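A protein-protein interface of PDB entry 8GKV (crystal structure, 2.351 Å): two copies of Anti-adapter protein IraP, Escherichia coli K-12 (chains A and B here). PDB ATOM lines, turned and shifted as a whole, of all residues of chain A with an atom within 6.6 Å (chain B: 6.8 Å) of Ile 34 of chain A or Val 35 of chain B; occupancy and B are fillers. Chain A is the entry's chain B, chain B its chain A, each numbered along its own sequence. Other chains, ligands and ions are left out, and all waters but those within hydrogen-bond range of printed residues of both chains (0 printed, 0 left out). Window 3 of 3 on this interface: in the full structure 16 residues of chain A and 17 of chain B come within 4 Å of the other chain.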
ATOM      1  N   GLU A  29       2.067  18.033   4.623  1.00  0.00           N
ATOM      2  CA  GLU A  29       3.205  18.230   5.521  1.00  0.00           C
ATOM      3  C   GLU A  29       4.336  19.028   4.847  1.00  0.00           C
ATOM      4  O   GLU A  29       4.781  20.073   5.365  1.00  0.00           O
ATOM      5  CB  GLU A  29       3.745  16.886   6.011  1.00  0.00           C
ATOM      6  CG  GLU A  29       3.141  16.401   7.326  1.00  0.00           C
ATOM      7  CD  GLU A  29       4.164  15.709   8.214  1.00  0.00           C
ATOM      8  OE1 GLU A  29       5.128  16.377   8.649  1.00  0.00           O
ATOM      9  OE2 GLU A  29       4.010  14.496   8.473  1.00  0.00           O
ATOM     10  N   ALA A  30       4.798  18.534   3.696  1.00  0.00           N
ATOM     11  CA  ALA A  30       5.866  19.209   2.954  1.00  0.00           C
ATOM     12  C   ALA A  30       5.537  20.691   2.730  1.00  0.00           C
ATOM     13  O   ALA A  30       6.326  21.589   3.065  1.00  0.00           O
ATOM     14  CB  ALA A  30       6.109  18.512   1.615  1.00  0.00           C
ATOM     15  N   LEU A  31       4.351  20.940   2.182  1.00  0.00           N
ATOM     16  CA  LEU A  31       3.929  22.297   1.850  1.00  0.00           C
ATOM     17  C   LEU A  31       3.812  23.172   3.090  1.00  0.00           C
ATOM     18  O   LEU A  31       4.136  24.357   3.046  1.00  0.00           O
ATOM     19  CB  LEU A  31       2.600  22.262   1.097  1.00  0.00           C
ATOM     20  CG  LEU A  31       2.724  21.610  -0.279  1.00  0.00           C
ATOM     21  CD1 LEU A  31       1.374  21.189  -0.829  1.00  0.00           C
ATOM     22  CD2 LEU A  31       3.417  22.555  -1.248  1.00  0.00           C
ATOM     23  N   GLU A  32       3.357  22.596   4.196  1.00  0.00           N
ATOM     24  CA  GLU A  32       3.268  23.350   5.441  1.00  0.00           C
ATOM     25  C   GLU A  32       4.666  23.759   5.910  1.00  0.00           C
ATOM     26  O   GLU A  32       4.897  24.934   6.243  1.00  0.00           O
ATOM     27  CB  GLU A  32       2.538  22.534   6.507  1.00  0.00           C
ATOM     28  CG  GLU A  32       1.030  22.531   6.320  1.00  0.00           C
ATOM     29  CD  GLU A  32       0.305  21.686   7.350  1.00  0.00           C
ATOM     30  OE1 GLU A  32       0.938  20.787   7.943  1.00  0.00           O
ATOM     31  OE2 GLU A  32      -0.902  21.921   7.569  1.00  0.00           O
ATOM     32  N   ILE A  33       5.603  22.810   5.900  1.00  0.00           N
ATOM     33  CA  ILE A  33       6.994  23.149   6.225  1.00  0.00           C
ATOM     34  C   ILE A  33       7.496  24.278   5.314  1.00  0.00           C
ATOM     35  O   ILE A  33       8.048  25.285   5.790  1.00  0.00           O
ATOM     36  CB  ILE A  33       7.926  21.927   6.108  1.00  0.00           C
ATOM     37  CG1 ILE A  33       7.589  20.929   7.217  1.00  0.00           C
ATOM     38  CG2 ILE A  33       9.388  22.353   6.238  1.00  0.00           C
ATOM     39  CD1 ILE A  33       8.248  19.578   7.071  1.00  0.00           C
ATOM     40  N   ILE A  34       7.284  24.121   4.009  1.00  0.00           N
ATOM     41  CA  ILE A  34       7.712  25.135   3.044  1.00  0.00           C
ATOM     42  C   ILE A  34       7.127  26.516   3.351  1.00  0.00           C
ATOM     43  O   ILE A  34       7.865  27.503   3.452  1.00  0.00           O
ATOM     44  CB  ILE A  34       7.325  24.736   1.606  1.00  0.00           C
ATOM     45  CG1 ILE A  34       8.199  23.568   1.147  1.00  0.00           C
ATOM     46  CG2 ILE A  34       7.488  25.916   0.650  1.00  0.00           C
ATOM     47  CD1 ILE A  34       7.791  22.957  -0.181  1.00  0.00           C
ATOM     48  N   VAL A  35       5.807  26.587   3.490  1.00  0.00           N
ATOM     49  CA  VAL A  35       5.139  27.859   3.732  1.00  0.00           C
ATOM     50  C   VAL A  35       5.674  28.473   5.022  1.00  0.00           C
ATOM     51  O   VAL A  35       5.970  29.667   5.069  1.00  0.00           O
ATOM     52  CB  VAL A  35       3.603  27.696   3.804  1.00  0.00           C
ATOM     53  CG1 VAL A  35       2.941  28.959   4.355  1.00  0.00           C
ATOM     54  CG2 VAL A  35       3.054  27.362   2.428  1.00  0.00           C
ATOM     55  N   THR A  36       5.815  27.654   6.061  1.00  0.00           N
ATOM     56  CA  THR A  36       6.419  28.130   7.302  1.00  0.00           C
ATOM     57  C   THR A  36       7.792  28.749   7.043  1.00  0.00           C
ATOM     58  O   THR A  36       8.077  29.860   7.505  1.00  0.00           O
ATOM     59  CB  THR A  36       6.562  26.995   8.332  1.00  0.00           C
ATOM     60  OG1 THR A  36       5.264  26.502   8.681  1.00  0.00           O
ATOM     61  CG2 THR A  36       7.265  27.490   9.598  1.00  0.00           C
ATOM     62  N   ALA A  37       8.643  28.033   6.309  1.00  0.00           N
ATOM     63  CA  ALA A  37       9.978  28.546   5.997  1.00  0.00           C
ATOM     64  C   ALA A  37       9.915  29.888   5.256  1.00  0.00           C
ATOM     65  O   ALA A  37      10.557  30.870   5.659  1.00  0.00           O
ATOM     66  CB  ALA A  37      10.756  27.528   5.176  1.00  0.00           C
ATOM     67  N   MET A  38       9.136  29.932   4.180  1.00  0.00           N
ATOM     68  CA  MET A  38       9.042  31.142   3.368  1.00  0.00           C
ATOM     69  C   MET A  38       8.439  32.302   4.154  1.00  0.00           C
ATOM     70  O   MET A  38       8.778  33.459   3.913  1.00  0.00           O
ATOM     71  CB  MET A  38       8.215  30.887   2.108  1.00  0.00           C
ATOM     72  CG  MET A  38       8.908  30.000   1.082  1.00  0.00           C
ATOM     73  SD  MET A  38       8.374  30.333  -0.607  1.00  0.00           S
ATOM     74  CE  MET A  38       6.646  29.873  -0.524  1.00  0.00           C
ATOM     75  N   LEU A  39       7.542  31.989   5.087  1.00  0.00           N
ATOM     76  CA  LEU A  39       6.985  33.007   5.972  1.00  0.00           C
ATOM     77  C   LEU A  39       8.054  33.538   6.918  1.00  0.00           C
ATOM     78  O   LEU A  39       8.238  34.750   7.034  1.00  0.00           O
ATOM     79  CB  LEU A  39       5.809  32.450   6.774  1.00  0.00           C
ATOM     80  CG  LEU A  39       4.507  32.256   5.997  1.00  0.00           C
ATOM     81  CD1 LEU A  39       3.555  31.406   6.808  1.00  0.00           C
ATOM     82  CD2 LEU A  39       3.865  33.594   5.656  1.00  0.00           C
ATOM     83  N   ALA B  30      -4.751  24.659  -1.937  1.00  0.00           N
ATOM     84  CA  ALA B  30      -4.602  25.925  -1.215  1.00  0.00           C
ATOM     85  C   ALA B  30      -3.126  26.275  -0.986  1.00  0.00           C
ATOM     86  O   ALA B  30      -2.639  27.356  -1.377  1.00  0.00           O
ATOM     87  CB  ALA B  30      -5.331  25.860   0.124  1.00  0.00           C
ATOM     88  N   LEU B  31      -2.417  25.342  -0.353  1.00  0.00           N
ATOM     89  CA  LEU B  31      -1.015  25.547  -0.018  1.00  0.00           C
ATOM     90  C   LEU B  31      -0.188  25.812  -1.270  1.00  0.00           C
ATOM     91  O   LEU B  31       0.678  26.688  -1.276  1.00  0.00           O
ATOM     92  CB  LEU B  31      -0.468  24.337   0.741  1.00  0.00           C
ATOM     93  CG  LEU B  31      -1.023  24.204   2.162  1.00  0.00           C
ATOM     94  CD1 LEU B  31      -0.740  22.828   2.747  1.00  0.00           C
ATOM     95  CD2 LEU B  31      -0.455  25.302   3.058  1.00  0.00           C
ATOM     96  N   GLU B  32      -0.470  25.070  -2.336  1.00  0.00           N
ATOM     97  CA  GLU B  32       0.251  25.262  -3.590  1.00  0.00           C
ATOM     98  C   GLU B  32       0.038  26.672  -4.136  1.00  0.00           C
ATOM     99  O   GLU B  32       0.999  27.340  -4.538  1.00  0.00           O
ATOM    100  CB  GLU B  32      -0.174  24.208  -4.612  1.00  0.00           C
ATOM    101  CG  GLU B  32       0.652  22.925  -4.519  1.00  0.00           C
ATOM    102  CD  GLU B  32       0.196  21.862  -5.492  1.00  0.00           C
ATOM    103  OE1 GLU B  32      -0.593  22.191  -6.402  1.00  0.00           O
ATOM    104  OE2 GLU B  32       0.622  20.696  -5.344  1.00  0.00           O
ATOM    105  N   ILE B  33      -1.212  27.133  -4.138  1.00  0.00           N
ATOM    106  CA  ILE B  33      -1.490  28.509  -4.555  1.00  0.00           C
ATOM    107  C   ILE B  33      -0.715  29.513  -3.691  1.00  0.00           C
ATOM    108  O   ILE B  33      -0.062  30.422  -4.220  1.00  0.00           O
ATOM    109  CB  ILE B  33      -2.997  28.818  -4.504  1.00  0.00           C
ATOM    110  CG1 ILE B  33      -3.713  28.005  -5.583  1.00  0.00           C
ATOM    111  CG2 ILE B  33      -3.255  30.306  -4.749  1.00  0.00           C
ATOM    112  CD1 ILE B  33      -5.184  27.791  -5.330  1.00  0.00           C
ATOM    113  N   ILE B  34      -0.778  29.349  -2.371  1.00  0.00           N
ATOM    114  CA  ILE B  34      -0.025  30.238  -1.475  1.00  0.00           C
ATOM    115  C   ILE B  34       1.488  30.266  -1.805  1.00  0.00           C
ATOM    116  O   ILE B  34       2.082  31.345  -2.021  1.00  0.00           O
ATOM    117  CB  ILE B  34      -0.227  29.829   0.001  1.00  0.00           C
ATOM    118  CG1 ILE B  34      -1.692  30.019   0.402  1.00  0.00           C
ATOM    119  CG2 ILE B  34       0.651  30.661   0.913  1.00  0.00           C
ATOM    120  CD1 ILE B  34      -2.059  29.447   1.765  1.00  0.00           C
ATOM    121  N   VAL B  35       2.102  29.084  -1.854  1.00  0.00           N
ATOM    122  CA  VAL B  35       3.529  28.971  -2.164  1.00  0.00           C
ATOM    123  C   VAL B  35       3.848  29.650  -3.493  1.00  0.00           C
ATOM    124  O   VAL B  35       4.782  30.453  -3.583  1.00  0.00           O
ATOM    125  CB  VAL B  35       3.989  27.495  -2.232  1.00  0.00           C
ATOM    126  CG1 VAL B  35       5.394  27.381  -2.819  1.00  0.00           C
ATOM    127  CG2 VAL B  35       3.942  26.850  -0.857  1.00  0.00           C
ATOM    128  N   THR B  36       3.070  29.323  -4.520  1.00  0.00           N
ATOM    129  CA  THR B  36       3.243  29.938  -5.831  1.00  0.00           C
ATOM    130  C   THR B  36       3.191  31.459  -5.730  1.00  0.00           C
ATOM    131  O   THR B  36       4.042  32.156  -6.294  1.00  0.00           O
ATOM    132  CB  THR B  36       2.169  29.453  -6.823  1.00  0.00           C
ATOM    133  OG1 THR B  36       2.365  28.058  -7.085  1.00  0.00           O
ATOM    134  CG2 THR B  36       2.244  30.225  -8.142  1.00  0.00           C
ATOM    135  N   ALA B  37       2.194  31.971  -5.013  1.00  0.00           N
ATOM    136  CA  ALA B  37       2.074  33.413  -4.827  1.00  0.00           C
ATOM    137  C   ALA B  37       3.352  33.987  -4.210  1.00  0.00           C
ATOM    138  O   ALA B  37       3.914  34.964  -4.719  1.00  0.00           O
ATOM    139  CB  ALA B  37       0.875  33.746  -3.960  1.00  0.00           C
ATOM    140  N   MET B  38       3.821  33.380  -3.121  1.00  0.00           N
ATOM    141  CA  MET B  38       5.041  33.890  -2.481  1.00  0.00           C
ATOM    142  C   MET B  38       6.295  33.770  -3.358  1.00  0.00           C
ATOM    143  O   MET B  38       7.176  34.632  -3.304  1.00  0.00           O
ATOM    144  CB  MET B  38       5.280  33.184  -1.153  1.00  0.00           C
ATOM    145  CG  MET B  38       4.292  33.615  -0.082  1.00  0.00           C
ATOM    146  SD  MET B  38       4.769  33.116   1.576  1.00  0.00           S
ATOM    147  CE  MET B  38       3.920  31.551   1.684  1.00  0.00           C
ATOM    148  N   LEU B  39       6.381  32.712  -4.156  1.00  0.00           N
ATOM    149  CA  LEU B  39       7.493  32.573  -5.095  1.00  0.00           C
ATOM    150  C   LEU B  39       7.438  33.662  -6.167  1.00  0.00           C
ATOM    151  O   LEU B  39       8.465  34.266  -6.503  1.00  0.00           O
ATOM    152  CB  LEU B  39       7.485  31.185  -5.739  1.00  0.00           C
ATOM    153  CG  LEU B  39       7.891  30.040  -4.810  1.00  0.00           C
ATOM    154  CD1 LEU B  39       7.486  28.704  -5.397  1.00  0.00           C
ATOM    155  CD2 LEU B  39       9.387  30.079  -4.579  1.00  0.00           C
ATOM    156  N   ARG B  40       6.246  33.912  -6.706  1.00  0.00           N
ATOM    157  CA  ARG B  40       6.065  35.023  -7.639  1.00  0.00           C
ATOM    158  C   ARG B  40       6.432  36.333  -6.949  1.00  0.00           C
ATOM    159  O   ARG B  40       7.001  37.231  -7.572  1.00  0.00           O
ATOM    160  CB  ARG B  40       4.629  35.084  -8.170  1.00  0.00           C
ATOM    161  CG  ARG B  40       4.336  34.090  -9.285  1.00  0.00           C
ATOM    162  CD  ARG B  40       2.937  34.291  -9.866  1.00  0.00           C
ATOM    163  NE  ARG B  40       2.790  35.581 -10.544  1.00  0.00           N
ATOM    164  CZ  ARG B  40       2.844  35.764 -11.863  1.00  0.00           C
ATOM    165  NH1 ARG B  40       3.039  34.742 -12.689  1.00  0.00           N
ATOM    166  NH2 ARG B  40       2.694  36.985 -12.363  1.00  0.00           N
ATOM    167  N   ASN B  41       6.105  36.441  -5.664  1.00  0.00           N
ATOM    168  CA  ASN B  41       6.539  37.589  -4.870  1.00  0.00           C
ATOM    169  C   ASN B  41       8.061  37.697  -4.797  1.00  0.00           C
ATOM    170  O   ASN B  41       8.616  38.780  -4.989  1.00  0.00           O
ATOM    171  CB  ASN B  41       5.955  37.518  -3.459  1.00  0.00           C
ATOM    172  CG  ASN B  41       4.795  38.465  -3.267  1.00  0.00           C
ATOM    173  OD1 ASN B  41       4.784  39.269  -2.336  1.00  0.00           O
ATOM    174  ND2 ASN B  41       3.820  38.392  -4.162  1.00  0.00           N
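Leu 31 of chain B touches its own counterpart, Leu 31 of chain A. Glu 32 of chain A touches Leu 31 of chain B, but with the chains exchanged Leu 31 of chain A does not touch Glu 32 of chain B (4.1 Å). Val 35 of chain A touches its own counterpart, Val 35 of chain B. Met 38 of chain B touches its own counterpart, Met 38 of chain A. 10 positions are printed for both chains. Of the 7 pairs that touch across the chains among the printed residues, 5 have their exchanged pair printed and touching as well.
Ile 34 of chain A touches one residue of chain B. Val 35 of chain B touches three residues of chain A. Printed residues of chain B within 4 Å of Leu 31 of chain A: Leu 31 (3.7 Å). Of the printed residues of chain B, Val 35 of chain A touches Val 35 (3.4 Å) and Met 38 (3.8 Å). The nearest residue of chain A that does not touch Val 35 of chain B is Leu 31 of chain A (4.3 Å).
Printed residues of chain A that touch a printed residue of chain B: Leu 31, Glu 32, Ile 34, Val 35 and Met 38. Of the 12 printed residues of chain B, 3 touch a printed residue of chain A. Hydrophobic or aromatic side chains of chain B that line the printed part of chain A: Leu 31, Val 35 and Met 38. Among the printed residues, 7 pairs touch across the chains. Among the printed residues, no Asp or Glu carboxylate lies within 4 Å of a Lys or Arg side-chain nitrogen of the other chain.
Among the printed residues, merely in contact across the chains: Leu 31 of chain A with Leu 31 of chain B (3.7 Å), Glu 32 of chain A with Leu 31 of chain B (3.998 Å), Ile 34 of chain A with Val 35 of chain B (3.96 Å), Val 35 of chain A with Val 35 of chain B (3.4 Å), Val 35 of chain A with Met 38 of chain B (3.8 Å), Met 38 of chain A with Val 35 of chain B (3.6 Å) and Met 38 of chain A with Met 38 of chain B (3.6 Å).
OG1 of Thr 36 of chain A lies within hydrogen-bond range of O of Glu 32 of chain A (2.9 Å).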
